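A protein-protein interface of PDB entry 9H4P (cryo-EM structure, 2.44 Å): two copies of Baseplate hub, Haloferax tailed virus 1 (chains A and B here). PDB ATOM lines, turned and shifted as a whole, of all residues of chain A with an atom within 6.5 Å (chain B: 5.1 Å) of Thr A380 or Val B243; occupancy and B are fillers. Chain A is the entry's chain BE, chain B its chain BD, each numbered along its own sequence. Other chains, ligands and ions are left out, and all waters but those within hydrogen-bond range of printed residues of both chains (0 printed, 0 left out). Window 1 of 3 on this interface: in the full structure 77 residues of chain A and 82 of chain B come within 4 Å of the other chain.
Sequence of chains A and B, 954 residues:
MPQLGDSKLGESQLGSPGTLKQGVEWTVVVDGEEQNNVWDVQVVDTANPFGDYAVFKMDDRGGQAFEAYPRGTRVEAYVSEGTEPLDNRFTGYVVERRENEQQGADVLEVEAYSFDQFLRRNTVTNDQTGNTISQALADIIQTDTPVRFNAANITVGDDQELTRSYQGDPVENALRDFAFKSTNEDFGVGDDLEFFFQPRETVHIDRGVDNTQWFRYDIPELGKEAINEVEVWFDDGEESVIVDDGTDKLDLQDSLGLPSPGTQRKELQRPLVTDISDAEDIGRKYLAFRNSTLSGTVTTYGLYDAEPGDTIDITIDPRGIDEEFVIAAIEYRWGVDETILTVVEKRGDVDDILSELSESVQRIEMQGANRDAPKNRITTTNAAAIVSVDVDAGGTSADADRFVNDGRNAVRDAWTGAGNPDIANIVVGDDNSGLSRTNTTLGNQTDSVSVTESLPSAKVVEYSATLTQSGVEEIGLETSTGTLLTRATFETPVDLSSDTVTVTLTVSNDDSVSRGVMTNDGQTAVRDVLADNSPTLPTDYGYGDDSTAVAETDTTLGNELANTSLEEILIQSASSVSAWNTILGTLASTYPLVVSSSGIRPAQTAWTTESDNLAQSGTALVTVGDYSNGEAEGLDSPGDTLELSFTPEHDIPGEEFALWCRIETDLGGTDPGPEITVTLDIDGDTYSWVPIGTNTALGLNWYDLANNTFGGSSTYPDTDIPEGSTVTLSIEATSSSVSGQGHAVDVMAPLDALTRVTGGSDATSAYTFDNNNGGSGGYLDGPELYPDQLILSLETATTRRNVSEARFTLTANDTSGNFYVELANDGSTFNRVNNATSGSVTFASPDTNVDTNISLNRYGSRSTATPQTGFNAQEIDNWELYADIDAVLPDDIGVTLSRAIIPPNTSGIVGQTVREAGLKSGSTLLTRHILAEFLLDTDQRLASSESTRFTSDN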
ATOM      1  N   ASN A 376      28.979   7.229 -29.383  1.00  0.00           N
ATOM      2  CA  ASN A 376      27.900   8.064 -28.872  1.00  0.00           C
ATOM      3  C   ASN A 376      28.056   8.143 -27.357  1.00  0.00           C
ATOM      4  O   ASN A 376      28.710   7.271 -26.789  1.00  0.00           O
ATOM      5  CB  ASN A 376      26.563   7.436 -29.267  1.00  0.00           C
ATOM      6  CG  ASN A 376      26.383   7.318 -30.766  1.00  0.00           C
ATOM      7  OD1 ASN A 376      26.114   8.289 -31.447  1.00  0.00           O
ATOM      8  ND2 ASN A 376      26.499   6.132 -31.303  1.00  0.00           N
ATOM      9  N   ARG A 377      27.469   9.119 -26.671  1.00  0.00           N
ATOM     10  CA  ARG A 377      27.654   9.276 -25.223  1.00  0.00           C
ATOM     11  C   ARG A 377      26.349   9.475 -24.472  1.00  0.00           C
ATOM     12  O   ARG A 377      25.517  10.278 -24.869  1.00  0.00           O
ATOM     13  CB  ARG A 377      28.673  10.394 -24.985  1.00  0.00           C
ATOM     14  CG  ARG A 377      28.900  10.686 -23.501  1.00  0.00           C
ATOM     15  CD  ARG A 377      30.095  11.608 -23.270  1.00  0.00           C
ATOM     16  NE  ARG A 377      31.336  10.858 -23.030  1.00  0.00           N
ATOM     17  CZ  ARG A 377      32.319  10.612 -23.865  1.00  0.00           C
ATOM     18  NH1 ARG A 377      33.369   9.991 -23.440  1.00  0.00           N
ATOM     19  NH2 ARG A 377      32.301  10.966 -25.111  1.00  0.00           N
ATOM     20  N   ILE A 378      26.206   8.789 -23.346  1.00  0.00           N
ATOM     21  CA  ILE A 378      25.167   9.007 -22.346  1.00  0.00           C
ATOM     22  C   ILE A 378      25.837   9.521 -21.084  1.00  0.00           C
ATOM     23  O   ILE A 378      26.682   8.827 -20.525  1.00  0.00           O
ATOM     24  CB  ILE A 378      24.389   7.719 -22.021  1.00  0.00           C
ATOM     25  CG1 ILE A 378      24.045   6.853 -23.234  1.00  0.00           C
ATOM     26  CG2 ILE A 378      23.124   8.066 -21.229  1.00  0.00           C
ATOM     27  CD1 ILE A 378      23.131   7.498 -24.276  1.00  0.00           C
ATOM     28  N   THR A 379      25.464  10.693 -20.587  1.00  0.00           N
ATOM     29  CA  THR A 379      25.987  11.185 -19.306  1.00  0.00           C
ATOM     30  C   THR A 379      25.037  10.800 -18.181  1.00  0.00           C
ATOM     31  O   THR A 379      23.831  10.966 -18.300  1.00  0.00           O
ATOM     32  CB  THR A 379      26.245  12.691 -19.309  1.00  0.00           C
ATOM     33  OG1 THR A 379      25.071  13.436 -19.498  1.00  0.00           O
ATOM     34  CG2 THR A 379      27.254  13.102 -20.373  1.00  0.00           C
ATOM     35  N   THR A 380      25.560  10.259 -17.085  1.00  0.00           N
ATOM     36  CA  THR A 380      24.760   9.871 -15.917  1.00  0.00           C
ATOM     37  C   THR A 380      24.917  10.925 -14.836  1.00  0.00           C
ATOM     38  O   THR A 380      26.036  11.244 -14.448  1.00  0.00           O
ATOM     39  CB  THR A 380      25.184   8.498 -15.390  1.00  0.00           C
ATOM     40  OG1 THR A 380      25.027   7.547 -16.412  1.00  0.00           O
ATOM     41  CG2 THR A 380      24.335   8.025 -14.217  1.00  0.00           C
ATOM     42  N   THR A 381      23.812  11.471 -14.337  1.00  0.00           N
ATOM     43  CA  THR A 381      23.802  12.583 -13.379  1.00  0.00           C
ATOM     44  C   THR A 381      22.732  12.370 -12.316  1.00  0.00           C
ATOM     45  O   THR A 381      21.693  11.779 -12.588  1.00  0.00           O
ATOM     46  CB  THR A 381      23.589  13.926 -14.093  1.00  0.00           C
ATOM     47  OG1 THR A 381      22.511  13.857 -14.985  1.00  0.00           O
ATOM     48  CG2 THR A 381      24.807  14.374 -14.891  1.00  0.00           C
ATOM     49  N   ASN A 382      22.968  12.837 -11.090  1.00  0.00           N
ATOM     50  CA  ASN A 382      22.056  12.670  -9.958  1.00  0.00           C
ATOM     51  C   ASN A 382      21.823  13.999  -9.251  1.00  0.00           C
ATOM     52  O   ASN A 382      22.775  14.681  -8.898  1.00  0.00           O
ATOM     53  CB  ASN A 382      22.634  11.671  -8.948  1.00  0.00           C
ATOM     54  CG  ASN A 382      22.784  10.273  -9.487  1.00  0.00           C
ATOM     55  OD1 ASN A 382      21.825   9.527  -9.573  1.00  0.00           O
ATOM     56  ND2 ASN A 382      23.977   9.862  -9.833  1.00  0.00           N
ATOM     57  N   HIS A 929      25.065  20.073 -12.815  1.00  0.00           N
ATOM     58  CA  HIS A 929      26.050  19.014 -12.595  1.00  0.00           C
ATOM     59  C   HIS A 929      27.371  19.358 -13.244  1.00  0.00           C
ATOM     60  O   HIS A 929      27.383  19.924 -14.331  1.00  0.00           O
ATOM     61  CB  HIS A 929      25.573  17.701 -13.206  1.00  0.00           C
ATOM     62  CG  HIS A 929      24.206  17.320 -12.761  1.00  0.00           C
ATOM     63  ND1 HIS A 929      23.901  16.638 -11.591  1.00  0.00           N
ATOM     64  CD2 HIS A 929      23.062  17.663 -13.398  1.00  0.00           C
ATOM     65  CE1 HIS A 929      22.567  16.592 -11.550  1.00  0.00           C
ATOM     66  NE2 HIS A 929      22.044  17.202 -12.614  1.00  0.00           N
ATOM     67  N   LEU A 931      30.693  17.553 -15.035  1.00  0.00           N
ATOM     68  CA  LEU A 931      30.973  16.353 -15.808  1.00  0.00           C
ATOM     69  C   LEU A 931      32.479  16.206 -16.009  1.00  0.00           C
ATOM     70  O   LEU A 931      33.194  17.194 -16.152  1.00  0.00           O
ATOM     71  CB  LEU A 931      30.244  16.446 -17.155  1.00  0.00           C
ATOM     72  CG  LEU A 931      28.724  16.603 -17.055  1.00  0.00           C
ATOM     73  CD1 LEU A 931      28.162  16.827 -18.444  1.00  0.00           C
ATOM     74  CD2 LEU A 931      28.069  15.365 -16.472  1.00  0.00           C
ATOM     75  N   ALA A 943      23.343  12.168 -25.116  1.00  0.00           N
ATOM     76  CA  ALA A 943      22.082  12.093 -24.387  1.00  0.00           C
ATOM     77  C   ALA A 943      22.258  12.110 -22.866  1.00  0.00           C
ATOM     78  O   ALA A 943      23.308  11.747 -22.341  1.00  0.00           O
ATOM     79  CB  ALA A 943      21.298  10.878 -24.868  1.00  0.00           C
ATOM     80  N   SER A 944      21.239  12.553 -22.138  1.00  0.00           N
ATOM     81  CA  SER A 944      21.238  12.569 -20.676  1.00  0.00           C
ATOM     82  C   SER A 944      20.753  11.255 -20.066  1.00  0.00           C
ATOM     83  O   SER A 944      20.052  10.462 -20.688  1.00  0.00           O
ATOM     84  CB  SER A 944      20.371  13.720 -20.166  1.00  0.00           C
ATOM     85  OG  SER A 944      19.005  13.502 -20.455  1.00  0.00           O
ATOM     86  N   SER A 945      21.056  11.053 -18.796  1.00  0.00           N
ATOM     87  CA  SER A 945      20.408  10.101 -17.899  1.00  0.00           C
ATOM     88  C   SER A 945      20.391  10.724 -16.516  1.00  0.00           C
ATOM     89  O   SER A 945      21.174  10.394 -15.634  1.00  0.00           O
ATOM     90  CB  SER A 945      21.094   8.743 -17.947  1.00  0.00           C
ATOM     91  OG  SER A 945      20.683   8.117 -19.140  1.00  0.00           O
ATOM     92  N   GLU A 946      19.529  11.723 -16.395  1.00  0.00           N
ATOM     93  CA  GLU A 946      19.401  12.606 -15.251  1.00  0.00           C
ATOM     94  C   GLU A 946      18.414  12.017 -14.245  1.00  0.00           C
ATOM     95  O   GLU A 946      17.207  12.117 -14.435  1.00  0.00           O
ATOM     96  CB  GLU A 946      18.922  13.941 -15.818  1.00  0.00           C
ATOM     97  CG  GLU A 946      18.521  15.018 -14.802  1.00  0.00           C
ATOM     98  CD  GLU A 946      19.682  15.880 -14.312  1.00  0.00           C
ATOM     99  OE1 GLU A 946      20.765  15.845 -14.934  1.00  0.00           O
ATOM    100  OE2 GLU A 946      19.486  16.636 -13.338  1.00  0.00           O
ATOM    101  N   SER A 947      18.901  11.408 -13.176  1.00  0.00           N
ATOM    102  CA  SER A 947      18.060  10.987 -12.063  1.00  0.00           C
ATOM    103  C   SER A 947      17.708  12.183 -11.187  1.00  0.00           C
ATOM    104  O   SER A 947      18.599  12.887 -10.716  1.00  0.00           O
ATOM    105  CB  SER A 947      18.766   9.932 -11.217  1.00  0.00           C
ATOM    106  OG  SER A 947      18.978   8.758 -11.970  1.00  0.00           O
ATOM    107  N   ASN B 228      33.074   3.314 -13.468  1.00  0.00           N
ATOM    108  CA  ASN B 228      32.442   4.592 -13.782  1.00  0.00           C
ATOM    109  C   ASN B 228      32.319   4.892 -15.276  1.00  0.00           C
ATOM    110  O   ASN B 228      31.796   5.935 -15.658  1.00  0.00           O
ATOM    111  CB  ASN B 228      33.167   5.671 -12.989  1.00  0.00           C
ATOM    112  CG  ASN B 228      34.650   5.737 -13.280  1.00  0.00           C
ATOM    113  OD1 ASN B 228      35.089   5.639 -14.411  1.00  0.00           O
ATOM    114  ND2 ASN B 228      35.471   5.911 -12.284  1.00  0.00           N
ATOM    115  N   GLU B 229      32.737   3.980 -16.140  1.00  0.00           N
ATOM    116  CA  GLU B 229      32.489   4.081 -17.565  1.00  0.00           C
ATOM    117  C   GLU B 229      32.214   2.703 -18.151  1.00  0.00           C
ATOM    118  O   GLU B 229      32.917   1.742 -17.862  1.00  0.00           O
ATOM    119  CB  GLU B 229      33.689   4.777 -18.205  1.00  0.00           C
ATOM    120  CG  GLU B 229      33.507   5.047 -19.696  1.00  0.00           C
ATOM    121  CD  GLU B 229      34.670   5.885 -20.236  1.00  0.00           C
ATOM    122  OE1 GLU B 229      34.901   7.004 -19.726  1.00  0.00           O
ATOM    123  OE2 GLU B 229      35.348   5.413 -21.173  1.00  0.00           O
ATOM    124  N   VAL B 230      31.215   2.585 -19.006  1.00  0.00           N
ATOM    125  CA  VAL B 230      30.960   1.364 -19.774  1.00  0.00           C
ATOM    126  C   VAL B 230      30.852   1.754 -21.225  1.00  0.00           C
ATOM    127  O   VAL B 230      30.152   2.704 -21.532  1.00  0.00           O
ATOM    128  CB  VAL B 230      29.692   0.646 -19.302  1.00  0.00           C
ATOM    129  CG1 VAL B 230      29.317  -0.528 -20.199  1.00  0.00           C
ATOM    130  CG2 VAL B 230      29.883   0.063 -17.910  1.00  0.00           C
ATOM    131  N   GLU B 231      31.486   1.032 -22.131  1.00  0.00           N
ATOM    132  CA  GLU B 231      31.250   1.210 -23.555  1.00  0.00           C
ATOM    133  C   GLU B 231      30.630  -0.046 -24.144  1.00  0.00           C
ATOM    134  O   GLU B 231      31.192  -1.130 -24.018  1.00  0.00           O
ATOM    135  CB  GLU B 231      32.530   1.664 -24.242  1.00  0.00           C
ATOM    136  CG  GLU B 231      32.238   2.061 -25.688  1.00  0.00           C
ATOM    137  CD  GLU B 231      33.390   2.785 -26.391  1.00  0.00           C
ATOM    138  OE1 GLU B 231      34.427   3.066 -25.744  1.00  0.00           O
ATOM    139  OE2 GLU B 231      33.251   3.099 -27.596  1.00  0.00           O
ATOM    140  N   VAL B 241      28.164   2.899 -27.899  1.00  0.00           N
ATOM    141  CA  VAL B 241      27.754   3.949 -26.967  1.00  0.00           C
ATOM    142  C   VAL B 241      28.550   3.867 -25.673  1.00  0.00           C
ATOM    143  O   VAL B 241      28.725   2.792 -25.113  1.00  0.00           O
ATOM    144  CB  VAL B 241      26.234   3.936 -26.751  1.00  0.00           C
ATOM    145  CG1 VAL B 241      25.688   2.654 -26.128  1.00  0.00           C
ATOM    146  CG2 VAL B 241      25.788   5.094 -25.869  1.00  0.00           C
ATOM    147  N   ILE B 242      29.000   5.007 -25.171  1.00  0.00           N
ATOM    148  CA  ILE B 242      29.691   5.157 -23.896  1.00  0.00           C
ATOM    149  C   ILE B 242      28.689   5.648 -22.862  1.00  0.00           C
ATOM    150  O   ILE B 242      28.070   6.687 -23.054  1.00  0.00           O
ATOM    151  CB  ILE B 242      30.851   6.162 -24.027  1.00  0.00           C
ATOM    152  CG1 ILE B 242      31.892   5.682 -25.052  1.00  0.00           C
ATOM    153  CG2 ILE B 242      31.526   6.370 -22.667  1.00  0.00           C
ATOM    154  CD1 ILE B 242      32.895   6.749 -25.474  1.00  0.00           C
ATOM    155  N   VAL B 243      28.548   4.939 -21.753  1.00  0.00           N
ATOM    156  CA  VAL B 243      27.752   5.342 -20.600  1.00  0.00           C
ATOM    157  C   VAL B 243      28.706   5.816 -19.524  1.00  0.00           C
ATOM    158  O   VAL B 243      29.622   5.100 -19.135  1.00  0.00           O
ATOM    159  CB  VAL B 243      26.871   4.191 -20.115  1.00  0.00           C
ATOM    160  CG1 VAL B 243      26.035   4.608 -18.911  1.00  0.00           C
ATOM    161  CG2 VAL B 243      25.913   3.748 -21.221  1.00  0.00           C
ATOM    162  N   ASP B 244      28.524   7.052 -19.085  1.00  0.00           N
ATOM    163  CA  ASP B 244      29.590   7.856 -18.502  1.00  0.00           C
ATOM    164  C   ASP B 244      29.160   8.447 -17.153  1.00  0.00           C
ATOM    165  O   ASP B 244      28.292   9.321 -17.099  1.00  0.00           O
ATOM    166  CB  ASP B 244      29.922   8.923 -19.559  1.00  0.00           C
ATOM    167  CG  ASP B 244      31.266   9.609 -19.364  1.00  0.00           C
ATOM    168  OD1 ASP B 244      31.816   9.570 -18.246  1.00  0.00           O
ATOM    169  OD2 ASP B 244      31.798  10.161 -20.352  1.00  0.00           O
ATOM    170  N   ASP B 245      29.724   7.958 -16.049  1.00  0.00           N
ATOM    171  CA  ASP B 245      29.448   8.446 -14.697  1.00  0.00           C
ATOM    172  C   ASP B 245      30.481   9.496 -14.261  1.00  0.00           C
ATOM    173  O   ASP B 245      31.517   9.191 -13.671  1.00  0.00           O
ATOM    174  CB  ASP B 245      29.360   7.261 -13.730  1.00  0.00           C
ATOM    175  CG  ASP B 245      28.963   7.666 -12.308  1.00  0.00           C
ATOM    176  OD1 ASP B 245      28.703   8.861 -12.053  1.00  0.00           O
ATOM    177  OD2 ASP B 245      28.871   6.762 -11.449  1.00  0.00           O
ATOM    178  N   GLY B 246      30.203  10.762 -14.573  1.00  0.00           N
ATOM    179  CA  GLY B 246      31.119  11.868 -14.318  1.00  0.00           C
ATOM    180  C   GLY B 246      31.452  12.067 -12.842  1.00  0.00           C
ATOM    181  O   GLY B 246      32.581  12.429 -12.524  1.00  0.00           O
ATOM    182  N   ALA B 279      21.128  -0.419 -25.976  1.00  0.00           N
ATOM    183  CA  ALA B 279      22.546  -0.483 -25.640  1.00  0.00           C
ATOM    184  C   ALA B 279      22.904   0.471 -24.489  1.00  0.00           C
ATOM    185  O   ALA B 279      23.641   0.105 -23.578  1.00  0.00           O
ATOM    186  CB  ALA B 279      23.359  -0.194 -26.897  1.00  0.00           C
ATOM    187  N   GLU B 280      22.235   1.625 -24.456  1.00  0.00           N
ATOM    188  CA  GLU B 280      22.435   2.535 -23.301  1.00  0.00           C
ATOM    189  C   GLU B 280      21.893   1.846 -22.042  1.00  0.00           C
ATOM    190  O   GLU B 280      22.648   1.761 -21.053  1.00  0.00           O
ATOM    191  CB  GLU B 280      21.719   3.867 -23.515  1.00  0.00           C
ATOM    192  CG  GLU B 280      21.497   4.625 -22.220  1.00  0.00           C
ATOM    193  CD  GLU B 280      20.450   5.721 -22.293  1.00  0.00           C
ATOM    194  OE1 GLU B 280      19.874   5.912 -23.382  1.00  0.00           O
ATOM    195  OE2 GLU B 280      20.214   6.379 -21.260  1.00  0.00           O
ATOM    196  N   GLY B 283      24.263  -0.586 -20.689  1.00  0.00           N
ATOM    197  CA  GLY B 283      25.375   0.082 -20.023  1.00  0.00           C
ATOM    198  C   GLY B 283      24.976   0.639 -18.661  1.00  0.00           C
ATOM    199  O   GLY B 283      25.689   0.431 -17.683  1.00  0.00           O
ATOM    200  N   ARG B 284      23.802   1.266 -18.544  1.00  0.00           N
ATOM    201  CA  ARG B 284      23.312   1.765 -17.254  1.00  0.00           C
ATOM    202  C   ARG B 284      23.022   0.642 -16.270  1.00  0.00           C
ATOM    203  O   ARG B 284      23.382   0.775 -15.108  1.00  0.00           O
ATOM    204  CB  ARG B 284      22.072   2.639 -17.424  1.00  0.00           C
ATOM    205  CG  ARG B 284      22.357   3.932 -18.194  1.00  0.00           C
ATOM    206  CD  ARG B 284      21.226   4.951 -18.081  1.00  0.00           C
ATOM    207  NE  ARG B 284      19.909   4.363 -18.372  1.00  0.00           N
ATOM    208  CZ  ARG B 284      18.987   4.019 -17.497  1.00  0.00           C
ATOM    209  NH1 ARG B 284      17.924   3.399 -17.898  1.00  0.00           N
ATOM    210  NH2 ARG B 284      19.094   4.261 -16.225  1.00  0.00           N
ATOM    211  N   LEU B 287      26.462  -0.566 -14.886  1.00  0.00           N
ATOM    212  CA  LEU B 287      26.896   0.339 -13.819  1.00  0.00           C
ATOM    213  C   LEU B 287      26.052   0.182 -12.554  1.00  0.00           C
ATOM    214  O   LEU B 287      26.602  -0.020 -11.481  1.00  0.00           O
ATOM    215  CB  LEU B 287      26.843   1.801 -14.287  1.00  0.00           C
ATOM    216  CG  LEU B 287      27.866   2.203 -15.351  1.00  0.00           C
ATOM    217  CD1 LEU B 287      27.695   3.679 -15.677  1.00  0.00           C
ATOM    218  CD2 LEU B 287      29.296   2.004 -14.877  1.00  0.00           C
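Asn A376 touches Val B241 (O to CA, 3.5 Å). Arg A377 touches Ile B242. Ile A378 touches Val B241. CA of Val B243 touches O of Ile A378, at 3.6 Å. Glu B280 touches Ile A378 (OE2 to CG2, 3.4 Å). Thr A379 touches Asp B244. CG1 of Val B243 touches OG1 of Thr A380 (3.99 Å). CD of Arg B284 touches OG of Ser A945, 3.4 Å away.
No position is printed for both chains. Of the 14 pairs that touch across the chains among the printed residues, none has its exchanged pair printed and touching as well.
Of the printed residues of chain B, Thr A379 touches Asp B244 (3.7 Å). Printed residues of chain B within 4 Å of Thr A380: Val B243 and Asp B244. Of the printed residues of chain B, Ser A945 touches Glu B280 and Arg B284. Printed residues of chain A within 4 Å of Val B243: Ile A378 and Thr A380. Asp B245 touches none of the printed residues of chain A. The nearest printed residue of chain B that does not touch Thr A380 is Gly B246 (4.2 Å).
OE2 of Glu B280 lies within hydrogen-bond range of OG of Ser A945 (2.8 Å). N of Ile A378 lies within hydrogen-bond range of O of Ile B242, 2.8 Å away. O of Ile A378 lies within hydrogen-bond range of N of Asp B244. The side-chain carboxylate (OD2) of Asp B244 lies within salt-bridge range of the guanidinium group (NE) of Arg A377 (2.8 Å). The backbone carbonyl oxygen (O) of Asn A376 sits at hydrogen-bond distance from the backbone NH (N) of Ile B242 (2.8 Å). N of Thr A380 sits at hydrogen-bond distance from O of Asp B244.
Of the 14 printed residues of chain A, 6 touch a printed residue of chain B. Hydrophobic or aromatic side chains of chain A within 4 Å of the printed part of chain B: Ile A378. Of the 15 printed residues of chain B, 6 touch a printed residue of chain A. Hydrophobic or aromatic side chains of chain B within 4 Å of the printed part of chain A: Val B241, Ile B242 and Val B243. Among the printed residues, Asp or Glu carboxylates within 4 Å of a Lys or Arg side-chain nitrogen of the other chain: Arg A377 with Asp B244 (2.8 Å).
The backbone NH (N) of Ala A943 lies within hydrogen-bond range of the backbone carbonyl oxygen (O) of Arg A377, at 2.9 Å. The backbone carbonyl oxygen of Ala A943 sits at hydrogen-bond distance from the backbone NH of Thr A379 (3.0 Å). The backbone carbonyl oxygen (O) of Val B230 lies within hydrogen-bond range of the backbone NH (N) of Val B243. O of Ser A945 lies within hydrogen-bond range of N of Thr A381 (3.1 Å). The side-chain carboxylate (OE2) of Glu B280 is in salt-bridge range of the guanidinium group (NE) of Arg B284 (3.5 Å). The backbone NH of Ser A945 lies within hydrogen-bond range of the backbone carbonyl oxygen of Thr A379 (2.8 Å).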
